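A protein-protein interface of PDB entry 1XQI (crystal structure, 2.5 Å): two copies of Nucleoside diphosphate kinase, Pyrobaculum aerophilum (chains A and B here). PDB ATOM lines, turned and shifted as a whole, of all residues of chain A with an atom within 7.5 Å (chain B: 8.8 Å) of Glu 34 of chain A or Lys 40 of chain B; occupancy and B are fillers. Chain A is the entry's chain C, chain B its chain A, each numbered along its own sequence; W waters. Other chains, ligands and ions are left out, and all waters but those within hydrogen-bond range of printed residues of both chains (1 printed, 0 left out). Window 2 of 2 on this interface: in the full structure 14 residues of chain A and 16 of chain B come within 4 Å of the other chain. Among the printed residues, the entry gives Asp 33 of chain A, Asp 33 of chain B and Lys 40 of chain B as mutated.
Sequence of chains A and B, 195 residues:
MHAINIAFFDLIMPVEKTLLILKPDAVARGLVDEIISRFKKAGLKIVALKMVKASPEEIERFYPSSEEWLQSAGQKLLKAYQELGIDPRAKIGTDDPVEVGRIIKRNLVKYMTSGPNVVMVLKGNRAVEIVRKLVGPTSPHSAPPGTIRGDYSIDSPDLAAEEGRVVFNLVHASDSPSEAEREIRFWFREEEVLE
NZ of Lys 40 of chain B lies within hydrogen-bond range of O of Gly 30 of chain A, 3.0 Å away. NZ of Lys 40 of chain B is in salt-bridge range of OD1 of Asp 33 of chain A (2.7 Å). The side-chain amino group (NZ) of Lys 40 of chain B lies within salt-bridge range of the side-chain carboxylate (OE2) of Glu 34 of chain A (3.4 Å).
O of Asp 33 of chain A touches CB of Asp 33 of chain B, 3.4 Å away. Ile 36 of chain B touches Asp 33 of chain A. CB of Ser 37 of chain B touches OD2 of Asp 33 of chain A, 3.3 Å away. CG2 of Ile 36 of chain A touches CB of Asp 33 of chain B (3.7 Å). Ser 37 of chain A touches Asp 33 of chain B (CB to OD1, 3.0 Å).
Of the printed residues of chain B, Gly 30 of chain A touches Lys 40. Of chain B, only Asp 33, Ile 36, Ser 37 and Lys 40 come within 4 Å of Asp 33 of chain A. Glu 34 of chain A touches one residue of chain B. Printed residues of chain B within 4 Å of Ile 36 of chain A: Asp 33 (3.7 Å). Printed residues of chain A within 4 Å of Asp 33 of chain B: Asp 33 (3.4 Å), Ile 36 (3.7 Å) and Ser 37 (3.0 Å). Printed residues of chain A within 4 Å of Ile 36 of chain B: Asp 33. Printed residues of chain A within 4 Å of Ser 37 of chain B: Asp 33. Lys 40 of chain B touches just these residues of chain A: Gly 30 (3.0 Å), Asp 33 (2.7 Å) and Glu 34 (3.4 Å). The nearest residue of chain B that does not touch Glu 34 of chain A is Asp 33 of chain B (5.4 Å). The nearest printed residue of chain A that does not touch Ser 37 of chain B is Glu 34 of chain A (6.2 Å).
Of the 16 printed residues of chain A, 5 touch a printed residue of chain B. Hydrophobic or aromatic side chains of chain A within 4 Å of the printed part of chain B: Ile 36. Along chain A the printed residues that touch a printed residue of chain B span positions 30 to 37. Of the 19 printed residues of chain B, 4 touch a printed residue of chain A. Hydrophobic or aromatic side chains of chain B that line the printed part of chain A: Ile 36. Among the printed residues, 8 pairs touch across the chains.
Asp 33 of chain A touches its own counterpart, Asp 33 of chain B. Asp 33 of chain A touches Ile 36 of chain B, and with the chains exchanged Ile 36 of chain A touches Asp 33 of chain B. Asp 33 of chain A touches Ser 37 of chain B, and with the chains exchanged Ser 37 of chain A touches Asp 33 of chain B. Positions printed for both chains: 32, 33, 34, 35, 36, 37, 38, 39 and 41.
Water W1 bridges OD2 of Asp 33 of chain A (2.5 Å) and OD1 of Asp 33 of chain B (2.6 Å).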
ATOM      1  N   LEU A  22     -33.685  39.170 -19.927  1.00  0.00           N
ATOM      2  CA  LEU A  22     -33.261  38.840 -21.263  1.00  0.00           C
ATOM      3  C   LEU A  22     -34.515  38.710 -22.134  1.00  0.00           C
ATOM      4  O   LEU A  22     -35.362  37.813 -21.937  1.00  0.00           O
ATOM      5  CB  LEU A  22     -32.424  37.554 -21.291  1.00  0.00           C
ATOM      6  CG  LEU A  22     -31.214  37.580 -20.371  1.00  0.00           C
ATOM      7  CD1 LEU A  22     -30.595  36.232 -20.294  1.00  0.00           C
ATOM      8  CD2 LEU A  22     -30.167  38.579 -20.846  1.00  0.00           C
ATOM      9  N   VAL A  27     -32.675  35.599 -25.715  1.00  0.00           N
ATOM     10  CA  VAL A  27     -32.852  34.196 -25.387  1.00  0.00           C
ATOM     11  C   VAL A  27     -32.767  33.317 -26.639  1.00  0.00           C
ATOM     12  O   VAL A  27     -32.031  32.317 -26.667  1.00  0.00           O
ATOM     13  CB  VAL A  27     -34.195  33.958 -24.737  1.00  0.00           C
ATOM     14  CG1 VAL A  27     -34.462  32.442 -24.582  1.00  0.00           C
ATOM     15  CG2 VAL A  27     -34.321  34.749 -23.399  1.00  0.00           C
ATOM     16  N   ARG A  29     -31.244  33.745 -29.420  1.00  0.00           N
ATOM     17  CA  ARG A  29     -29.884  33.686 -29.925  1.00  0.00           C
ATOM     18  C   ARG A  29     -28.884  32.932 -29.016  1.00  0.00           C
ATOM     19  O   ARG A  29     -27.706  32.866 -29.365  1.00  0.00           O
ATOM     20  CB  ARG A  29     -29.331  35.099 -30.155  1.00  0.00           C
ATOM     21  CG  ARG A  29     -29.966  35.922 -31.315  1.00  0.00           C
ATOM     22  CD  ARG A  29     -28.907  36.818 -31.965  1.00  0.00           C
ATOM     23  NE  ARG A  29     -28.704  38.020 -31.202  1.00  0.00           N
ATOM     24  CZ  ARG A  29     -27.540  38.618 -30.961  1.00  0.00           C
ATOM     25  NH1 ARG A  29     -26.404  38.165 -31.429  1.00  0.00           N
ATOM     26  NH2 ARG A  29     -27.545  39.718 -30.245  1.00  0.00           N
ATOM     27  N   GLY A  30     -29.326  32.383 -27.875  1.00  0.00           N
ATOM     28  CA  GLY A  30     -28.463  31.643 -26.976  1.00  0.00           C
ATOM     29  C   GLY A  30     -27.596  32.487 -26.050  1.00  0.00           C
ATOM     30  O   GLY A  30     -26.552  32.035 -25.588  1.00  0.00           O
ATOM     31  N   LEU A  31     -28.029  33.695 -25.723  1.00  0.00           N
ATOM     32  CA  LEU A  31     -27.184  34.593 -24.970  1.00  0.00           C
ATOM     33  C   LEU A  31     -27.345  34.509 -23.469  1.00  0.00           C
ATOM     34  O   LEU A  31     -26.691  35.248 -22.732  1.00  0.00           O
ATOM     35  CB  LEU A  31     -27.366  36.053 -25.434  1.00  0.00           C
ATOM     36  CG  LEU A  31     -27.016  36.315 -26.900  1.00  0.00           C
ATOM     37  CD1 LEU A  31     -26.992  37.833 -27.186  1.00  0.00           C
ATOM     38  CD2 LEU A  31     -25.711  35.576 -27.368  1.00  0.00           C
ATOM     39  N   VAL A  32     -28.229  33.653 -23.009  1.00  0.00           N
ATOM     40  CA  VAL A  32     -28.431  33.543 -21.595  1.00  0.00           C
ATOM     41  C   VAL A  32     -27.134  33.251 -20.850  1.00  0.00           C
ATOM     42  O   VAL A  32     -26.817  33.956 -19.893  1.00  0.00           O
ATOM     43  CB  VAL A  32     -29.552  32.530 -21.212  1.00  0.00           C
ATOM     44  CG1 VAL A  32     -29.649  32.448 -19.762  1.00  0.00           C
ATOM     45  CG2 VAL A  32     -30.894  33.038 -21.734  1.00  0.00           C
ATOM     46  N   ASP A  33     -26.385  32.241 -21.269  1.00  0.00           N
ATOM     47  CA  ASP A  33     -25.224  31.867 -20.491  1.00  0.00           C
ATOM     48  C   ASP A  33     -24.097  32.923 -20.631  1.00  0.00           C
ATOM     49  O   ASP A  33     -23.357  33.204 -19.683  1.00  0.00           O
ATOM     50  CB  ASP A  33     -24.763  30.453 -20.851  1.00  0.00           C
ATOM     51  CG  ASP A  33     -23.878  30.434 -22.068  1.00  0.00           C
ATOM     52  OD1 ASP A  33     -24.376  30.366 -23.238  1.00  0.00           O
ATOM     53  OD2 ASP A  33     -22.653  30.542 -21.829  1.00  0.00           O
ATOM     54  N   GLU A  34     -23.987  33.526 -21.808  1.00  0.00           N
ATOM     55  CA  GLU A  34     -22.941  34.540 -22.056  1.00  0.00           C
ATOM     56  C   GLU A  34     -23.181  35.761 -21.197  1.00  0.00           C
ATOM     57  O   GLU A  34     -22.247  36.294 -20.574  1.00  0.00           O
ATOM     58  CB  GLU A  34     -22.835  34.900 -23.538  1.00  0.00           C
ATOM     59  CG  GLU A  34     -21.591  34.326 -24.167  1.00  0.00           C
ATOM     60  CD  GLU A  34     -21.863  33.681 -25.495  1.00  0.00           C
ATOM     61  OE1 GLU A  34     -22.833  34.114 -26.167  1.00  0.00           O
ATOM     62  OE2 GLU A  34     -21.119  32.737 -25.875  1.00  0.00           O
ATOM     63  N   ILE A  35     -24.450  36.148 -21.091  1.00  0.00           N
ATOM     64  CA  ILE A  35     -24.828  37.238 -20.199  1.00  0.00           C
ATOM     65  C   ILE A  35     -24.753  36.874 -18.716  1.00  0.00           C
ATOM     66  O   ILE A  35     -24.297  37.676 -17.891  1.00  0.00           O
ATOM     67  CB  ILE A  35     -26.171  37.772 -20.616  1.00  0.00           C
ATOM     68  CG1 ILE A  35     -26.029  38.383 -22.004  1.00  0.00           C
ATOM     69  CG2 ILE A  35     -26.734  38.753 -19.605  1.00  0.00           C
ATOM     70  CD1 ILE A  35     -27.323  38.863 -22.573  1.00  0.00           C
ATOM     71  N   ILE A  36     -25.128  35.660 -18.347  1.00  0.00           N
ATOM     72  CA  ILE A  36     -24.980  35.295 -16.950  1.00  0.00           C
ATOM     73  C   ILE A  36     -23.505  35.342 -16.561  1.00  0.00           C
ATOM     74  O   ILE A  36     -23.158  35.768 -15.452  1.00  0.00           O
ATOM     75  CB  ILE A  36     -25.601  33.921 -16.621  1.00  0.00           C
ATOM     76  CG1 ILE A  36     -27.127  34.026 -16.601  1.00  0.00           C
ATOM     77  CG2 ILE A  36     -25.095  33.367 -15.251  1.00  0.00           C
ATOM     78  CD1 ILE A  36     -27.834  32.659 -16.651  1.00  0.00           C
ATOM     79  N   SER A  37     -22.633  34.908 -17.468  1.00  0.00           N
ATOM     80  CA  SER A  37     -21.192  34.795 -17.154  1.00  0.00           C
ATOM     81  C   SER A  37     -20.601  36.177 -16.793  1.00  0.00           C
ATOM     82  O   SER A  37     -19.712  36.314 -15.950  1.00  0.00           O
ATOM     83  CB  SER A  37     -20.438  34.159 -18.333  1.00  0.00           C
ATOM     84  OG  SER A  37     -19.044  34.398 -18.200  1.00  0.00           O
ATOM     85  N   ARG A  38     -21.095  37.217 -17.450  1.00  0.00           N
ATOM     86  CA  ARG A  38     -20.603  38.533 -17.144  1.00  0.00           C
ATOM     87  C   ARG A  38     -20.968  39.023 -15.769  1.00  0.00           C
ATOM     88  O   ARG A  38     -20.125  39.601 -15.113  1.00  0.00           O
ATOM     89  CB  ARG A  38     -21.016  39.511 -18.212  1.00  0.00           C
ATOM     90  CG  ARG A  38     -20.515  39.053 -19.537  1.00  0.00           C
ATOM     91  CD  ARG A  38     -20.128  40.220 -20.304  1.00  0.00           C
ATOM     92  NE  ARG A  38     -19.636  39.884 -21.625  1.00  0.00           N
ATOM     93  CZ  ARG A  38     -19.367  40.805 -22.538  1.00  0.00           C
ATOM     94  NH1 ARG A  38     -19.573  42.097 -22.243  1.00  0.00           N
ATOM     95  NH2 ARG A  38     -18.914  40.434 -23.731  1.00  0.00           N
ATOM     96  N   PHE A  39     -22.176  38.751 -15.295  1.00  0.00           N
ATOM     97  CA  PHE A  39     -22.558  39.189 -13.926  1.00  0.00           C
ATOM     98  C   PHE A  39     -21.830  38.430 -12.844  1.00  0.00           C
ATOM     99  O   PHE A  39     -21.335  39.035 -11.874  1.00  0.00           O
ATOM    100  CB  PHE A  39     -24.045  39.069 -13.719  1.00  0.00           C
ATOM    101  CG  PHE A  39     -24.817  39.867 -14.701  1.00  0.00           C
ATOM    102  CD1 PHE A  39     -25.825  39.284 -15.468  1.00  0.00           C
ATOM    103  CD2 PHE A  39     -24.491  41.212 -14.925  1.00  0.00           C
ATOM    104  CE1 PHE A  39     -26.533  40.065 -16.402  1.00  0.00           C
ATOM    105  CE2 PHE A  39     -25.188  41.990 -15.828  1.00  0.00           C
ATOM    106  CZ  PHE A  39     -26.220  41.424 -16.564  1.00  0.00           C
ATOM    107  N   LYS A  41     -18.876  36.983 -13.091  1.00  0.00           N
ATOM    108  CA  LYS A  41     -17.491  37.320 -13.021  1.00  0.00           C
ATOM    109  C   LYS A  41     -17.315  38.614 -12.270  1.00  0.00           C
ATOM    110  O   LYS A  41     -16.286  38.826 -11.631  1.00  0.00           O
ATOM    111  CB  LYS A  41     -16.875  37.370 -14.427  1.00  0.00           C
ATOM    112  CG  LYS A  41     -16.679  36.006 -15.012  1.00  0.00           C
ATOM    113  CD  LYS A  41     -16.127  36.127 -16.434  1.00  0.00           C
ATOM    114  CE  LYS A  41     -15.828  34.722 -17.031  1.00  0.00           C
ATOM    115  NZ  LYS A  41     -15.376  33.853 -15.887  1.00  0.00           N
ATOM    116  N   ILE A 148     -22.407  44.728 -22.654  1.00  0.00           N
ATOM    117  CA  ILE A 148     -23.224  43.656 -23.185  1.00  0.00           C
ATOM    118  C   ILE A 148     -23.894  44.141 -24.506  1.00  0.00           C
ATOM    119  O   ILE A 148     -23.933  43.378 -25.497  1.00  0.00           O
ATOM    120  CB  ILE A 148     -24.231  43.138 -22.099  1.00  0.00           C
ATOM    121  CG1 ILE A 148     -23.469  42.419 -20.964  1.00  0.00           C
ATOM    122  CG2 ILE A 148     -25.345  42.294 -22.688  1.00  0.00           C
ATOM    123  CD1 ILE A 148     -24.277  42.115 -19.706  1.00  0.00           C
ATOM    124  N   TYR A 152     -22.782  42.415 -28.146  1.00  0.00           N
ATOM    125  CA  TYR A 152     -23.757  41.422 -28.641  1.00  0.00           C
ATOM    126  C   TYR A 152     -24.865  41.910 -29.518  1.00  0.00           C
ATOM    127  O   TYR A 152     -25.813  41.175 -29.744  1.00  0.00           O
ATOM    128  CB  TYR A 152     -24.399  40.629 -27.498  1.00  0.00           C
ATOM    129  CG  TYR A 152     -23.405  39.839 -26.701  1.00  0.00           C
ATOM    130  CD1 TYR A 152     -22.875  40.326 -25.519  1.00  0.00           C
ATOM    131  CD2 TYR A 152     -23.001  38.609 -27.143  1.00  0.00           C
ATOM    132  CE1 TYR A 152     -21.941  39.584 -24.801  1.00  0.00           C
ATOM    133  CE2 TYR A 152     -22.106  37.864 -26.444  1.00  0.00           C
ATOM    134  CZ  TYR A 152     -21.563  38.346 -25.288  1.00  0.00           C
ATOM    135  OH  TYR A 152     -20.644  37.544 -24.656  1.00  0.00           O
ATOM    136  N   VAL B  32     -23.746  27.640 -13.345  1.00  0.00           N
ATOM    137  CA  VAL B  32     -24.935  27.606 -14.134  1.00  0.00           C
ATOM    138  C   VAL B  32     -24.602  27.947 -15.573  1.00  0.00           C
ATOM    139  O   VAL B  32     -25.113  27.317 -16.459  1.00  0.00           O
ATOM    140  CB  VAL B  32     -26.067  28.502 -13.539  1.00  0.00           C
ATOM    141  CG1 VAL B  32     -27.174  28.715 -14.535  1.00  0.00           C
ATOM    142  CG2 VAL B  32     -26.645  27.816 -12.359  1.00  0.00           C
ATOM    143  N   ASP B  33     -23.768  28.947 -15.811  1.00  0.00           N
ATOM    144  CA  ASP B  33     -23.573  29.407 -17.155  1.00  0.00           C
ATOM    145  C   ASP B  33     -22.665  28.427 -17.901  1.00  0.00           C
ATOM    146  O   ASP B  33     -22.901  28.110 -19.042  1.00  0.00           O
ATOM    147  CB  ASP B  33     -23.083  30.860 -17.180  1.00  0.00           C
ATOM    148  CG  ASP B  33     -21.595  31.014 -16.794  1.00  0.00           C
ATOM    149  OD1 ASP B  33     -20.780  31.203 -17.726  1.00  0.00           O
ATOM    150  OD2 ASP B  33     -21.229  30.948 -15.589  1.00  0.00           O
ATOM    151  N   GLU B  34     -21.670  27.887 -17.225  1.00  0.00           N
ATOM    152  CA  GLU B  34     -20.757  26.979 -17.869  1.00  0.00           C
ATOM    153  C   GLU B  34     -21.509  25.754 -18.403  1.00  0.00           C
ATOM    154  O   GLU B  34     -21.351  25.335 -19.582  1.00  0.00           O
ATOM    155  CB  GLU B  34     -19.632  26.603 -16.906  1.00  0.00           C
ATOM    156  CG  GLU B  34     -18.305  27.296 -17.249  1.00  0.00           C
ATOM    157  CD  GLU B  34     -17.773  28.170 -16.144  1.00  0.00           C
ATOM    158  OE1 GLU B  34     -16.901  29.007 -16.424  1.00  0.00           O
ATOM    159  OE2 GLU B  34     -18.203  28.021 -14.987  1.00  0.00           O
ATOM    160  N   ILE B  35     -22.383  25.214 -17.547  1.00  0.00           N
ATOM    161  CA  ILE B  35     -23.220  24.030 -17.892  1.00  0.00           C
ATOM    162  C   ILE B  35     -24.254  24.325 -19.012  1.00  0.00           C
ATOM    163  O   ILE B  35     -24.428  23.531 -19.953  1.00  0.00           O
ATOM    164  CB  ILE B  35     -23.866  23.462 -16.609  1.00  0.00           C
ATOM    165  CG1 ILE B  35     -22.753  22.952 -15.690  1.00  0.00           C
ATOM    166  CG2 ILE B  35     -24.948  22.391 -16.917  1.00  0.00           C
ATOM    167  CD1 ILE B  35     -23.222  22.081 -14.528  1.00  0.00           C
ATOM    168  N   ILE B  36     -24.945  25.455 -18.896  1.00  0.00           N
ATOM    169  CA  ILE B  36     -25.834  25.887 -19.938  1.00  0.00           C
ATOM    170  C   ILE B  36     -25.050  26.000 -21.245  1.00  0.00           C
ATOM    171  O   ILE B  36     -25.529  25.539 -22.290  1.00  0.00           O
ATOM    172  CB  ILE B  36     -26.517  27.190 -19.579  1.00  0.00           C
ATOM    173  CG1 ILE B  36     -27.507  26.916 -18.443  1.00  0.00           C
ATOM    174  CG2 ILE B  36     -27.279  27.785 -20.805  1.00  0.00           C
ATOM    175  CD1 ILE B  36     -28.278  28.143 -18.008  1.00  0.00           C
ATOM    176  N   SER B  37     -23.829  26.539 -21.212  1.00  0.00           N
ATOM    177  CA  SER B  37     -23.068  26.628 -22.456  1.00  0.00           C
ATOM    178  C   SER B  37     -22.827  25.267 -23.194  1.00  0.00           C
ATOM    179  O   SER B  37     -22.900  25.186 -24.420  1.00  0.00           O
ATOM    180  CB  SER B  37     -21.775  27.411 -22.253  1.00  0.00           C
ATOM    181  OG  SER B  37     -20.865  27.097 -23.288  1.00  0.00           O
ATOM    182  N   ARG B  38     -22.546  24.199 -22.456  1.00  0.00           N
ATOM    183  CA  ARG B  38     -22.313  22.899 -23.092  1.00  0.00           C
ATOM    184  C   ARG B  38     -23.561  22.408 -23.821  1.00  0.00           C
ATOM    185  O   ARG B  38     -23.440  21.794 -24.899  1.00  0.00           O
ATOM    186  CB  ARG B  38     -21.829  21.868 -22.098  1.00  0.00           C
ATOM    187  CG  ARG B  38     -21.003  22.463 -21.014  1.00  0.00           C
ATOM    188  CD  ARG B  38     -19.497  22.325 -21.180  1.00  0.00           C
ATOM    189  NE  ARG B  38     -19.111  20.970 -20.814  1.00  0.00           N
ATOM    190  CZ  ARG B  38     -17.956  20.588 -20.267  1.00  0.00           C
ATOM    191  NH1 ARG B  38     -16.959  21.450 -19.979  1.00  0.00           N
ATOM    192  NH2 ARG B  38     -17.816  19.293 -20.025  1.00  0.00           N
ATOM    193  N   PHE B  39     -24.752  22.707 -23.285  1.00  0.00           N
ATOM    194  CA  PHE B  39     -25.954  22.170 -23.887  1.00  0.00           C
ATOM    195  C   PHE B  39     -26.320  22.993 -25.128  1.00  0.00           C
ATOM    196  O   PHE B  39     -26.669  22.455 -26.172  1.00  0.00           O
ATOM    197  CB  PHE B  39     -27.097  22.107 -22.866  1.00  0.00           C
ATOM    198  CG  PHE B  39     -26.816  21.192 -21.678  1.00  0.00           C
ATOM    199  CD1 PHE B  39     -27.045  21.628 -20.366  1.00  0.00           C
ATOM    200  CD2 PHE B  39     -26.323  19.890 -21.860  1.00  0.00           C
ATOM    201  CE1 PHE B  39     -26.821  20.763 -19.261  1.00  0.00           C
ATOM    202  CE2 PHE B  39     -26.075  19.014 -20.761  1.00  0.00           C
ATOM    203  CZ  PHE B  39     -26.327  19.450 -19.461  1.00  0.00           C
ATOM    204  N   LYS B  40     -26.206  24.312 -25.018  1.00  0.00           N
ATOM    205  CA  LYS B  40     -26.426  25.222 -26.133  1.00  0.00           C
ATOM    206  C   LYS B  40     -25.487  24.850 -27.282  1.00  0.00           C
ATOM    207  O   LYS B  40     -25.898  24.808 -28.444  1.00  0.00           O
ATOM    208  CB  LYS B  40     -26.158  26.673 -25.714  1.00  0.00           C
ATOM    209  CG  LYS B  40     -25.948  27.614 -26.919  1.00  0.00           C
ATOM    210  CD  LYS B  40     -25.597  29.022 -26.523  1.00  0.00           C
ATOM    211  CE  LYS B  40     -24.102  29.256 -26.412  1.00  0.00           C
ATOM    212  NZ  LYS B  40     -23.861  30.663 -25.872  1.00  0.00           N
ATOM    213  N   LYS B  41     -24.225  24.554 -26.962  1.00  0.00           N
ATOM    214  CA  LYS B  41     -23.295  24.234 -28.016  1.00  0.00           C
ATOM    215  C   LYS B  41     -23.607  22.951 -28.729  1.00  0.00           C
ATOM    216  O   LYS B  41     -23.271  22.824 -29.884  1.00  0.00           O
ATOM    217  CB  LYS B  41     -21.849  24.290 -27.542  1.00  0.00           C
ATOM    218  CG  LYS B  41     -21.392  25.675 -27.551  1.00  0.00           C
ATOM    219  CD  LYS B  41     -20.207  25.905 -26.634  1.00  0.00           C
ATOM    220  CE  LYS B  41     -19.766  27.395 -26.795  1.00  0.00           C
ATOM    221  NZ  LYS B  41     -18.611  27.646 -25.938  1.00  0.00           N
ATOM    222  N   ALA B  42     -24.290  22.027 -28.076  1.00  0.00           N
ATOM    223  CA  ALA B  42     -24.565  20.726 -28.672  1.00  0.00           C
ATOM    224  C   ALA B  42     -25.776  20.801 -29.593  1.00  0.00           C
ATOM    225  O   ALA B  42     -25.994  19.912 -30.416  1.00  0.00           O
ATOM    226  CB  ALA B  42     -24.789  19.669 -27.576  1.00  0.00           C
ATOM    227  N   GLY B  43     -26.559  21.864 -29.452  1.00  0.00           N
ATOM    228  CA  GLY B  43     -27.779  21.963 -30.208  1.00  0.00           C
ATOM    229  C   GLY B  43     -29.025  21.705 -29.371  1.00  0.00           C
ATOM    230  O   GLY B  43     -30.096  21.671 -29.903  1.00  0.00           O
ATOM    231  N   LEU B  44     -28.928  21.499 -28.068  1.00  0.00           N
ATOM    232  CA  LEU B  44     -30.147  21.431 -27.260  1.00  0.00           C
ATOM    233  C   LEU B  44     -30.757  22.818 -26.970  1.00  0.00           C
ATOM    234  O   LEU B  44     -30.012  23.788 -26.733  1.00  0.00           O
ATOM    235  CB  LEU B  44     -29.859  20.695 -25.958  1.00  0.00           C
ATOM    236  CG  LEU B  44     -29.490  19.217 -26.108  1.00  0.00           C
ATOM    237  CD1 LEU B  44     -28.501  18.807 -25.019  1.00  0.00           C
ATOM    238  CD2 LEU B  44     -30.741  18.308 -26.157  1.00  0.00           C
ATOM    239  N   LYS B  45     -32.096  22.924 -26.989  1.00  0.00           N
ATOM    240  CA  LYS B  45     -32.749  24.187 -26.613  1.00  0.00           C
ATOM    241  C   LYS B  45     -33.234  24.074 -25.172  1.00  0.00           C
ATOM    242  O   LYS B  45     -33.727  23.015 -24.785  1.00  0.00           O
ATOM    243  CB  LYS B  45     -33.933  24.535 -27.588  1.00  0.00           C
ATOM    244  N   ILE B  46     -33.063  25.120 -24.354  1.00  0.00           N
ATOM    245  CA  ILE B  46     -33.705  25.199 -23.019  1.00  0.00           C
ATOM    246  C   ILE B  46     -35.156  25.664 -23.200  1.00  0.00           C
ATOM    247  O   ILE B  46     -35.383  26.741 -23.706  1.00  0.00           O
ATOM    248  CB  ILE B  46     -32.998  26.218 -22.096  1.00  0.00           C
ATOM    249  CG1 ILE B  46     -31.564  25.766 -21.786  1.00  0.00           C
ATOM    250  CG2 ILE B  46     -33.847  26.520 -20.808  1.00  0.00           C
ATOM    251  CD1 ILE B  46     -30.774  26.794 -20.945  1.00  0.00           C
ATOM    252  N   MET B 120     -33.969  22.729 -15.320  1.00  0.00           N
ATOM    253  CA  MET B 120     -34.160  23.097 -16.736  1.00  0.00           C
ATOM    254  C   MET B 120     -34.687  21.899 -17.493  1.00  0.00           C
ATOM    255  O   MET B 120     -34.510  20.733 -17.105  1.00  0.00           O
ATOM    256  CB  MET B 120     -32.854  23.701 -17.407  1.00  0.00           C
ATOM    257  CG  MET B 120     -31.661  22.735 -17.533  1.00  0.00           C
ATOM    258  SD  MET B 120     -30.154  23.557 -18.118  1.00  0.00           S
ATOM    259  CE  MET B 120     -29.890  24.391 -16.597  1.00  0.00           C
ATOM    260  N   LEU B 122     -34.485  20.358 -21.334  1.00  0.00           N
ATOM    261  CA  LEU B 122     -33.684  20.443 -22.535  1.00  0.00           C
ATOM    262  C   LEU B 122     -34.382  19.559 -23.555  1.00  0.00           C
ATOM    263  O   LEU B 122     -34.734  18.398 -23.244  1.00  0.00           O
ATOM    264  CB  LEU B 122     -32.254  19.926 -22.291  1.00  0.00           C
ATOM    265  CG  LEU B 122     -31.385  20.841 -21.424  1.00  0.00           C
ATOM    266  CD1 LEU B 122     -30.326  20.005 -20.724  1.00  0.00           C
ATOM    267  CD2 LEU B 122     -30.773  21.900 -22.310  1.00  0.00           C
ATOM    268  N   LYS B 123     -34.588  20.135 -24.741  1.00  0.00           N
ATOM    269  CA  LYS B 123     -35.257  19.531 -25.875  1.00  0.00           C
ATOM    270  C   LYS B 123     -34.264  19.353 -27.046  1.00  0.00           C
ATOM    271  O   LYS B 123     -33.493  20.272 -27.428  1.00  0.00           O
ATOM    272  CB  LYS B 123     -36.430  20.454 -26.314  1.00  0.00           C
ATOM    273  CG  LYS B 123     -37.371  19.893 -27.419  1.00  0.00           C
ATOM    274  CD  LYS B 123     -38.185  21.013 -28.064  1.00  0.00           C
ATOM    275  CE  LYS B 123     -39.264  20.521 -29.061  1.00  0.00           C
ATOM    276  NZ  LYS B 123     -40.590  20.412 -28.352  1.00  0.00           N
ATOM    277  N   LEU B 134     -23.262  13.759 -22.081  1.00  0.00           N
ATOM    278  CA  LEU B 134     -22.535  14.979 -21.768  1.00  0.00           C
ATOM    279  C   LEU B 134     -22.139  15.118 -20.282  1.00  0.00           C
ATOM    280  O   LEU B 134     -21.102  15.721 -19.963  1.00  0.00           O
ATOM    281  CB  LEU B 134     -23.337  16.192 -22.213  1.00  0.00           C
ATOM    282  CG  LEU B 134     -23.056  16.825 -23.573  1.00  0.00           C
ATOM    283  CD1 LEU B 134     -22.757  15.783 -24.601  1.00  0.00           C
ATOM    284  CD2 LEU B 134     -24.214  17.728 -24.051  1.00  0.00           C
HETATM  285  O   HOH W   1     -20.698  30.666 -20.277  1.00  0.00           O
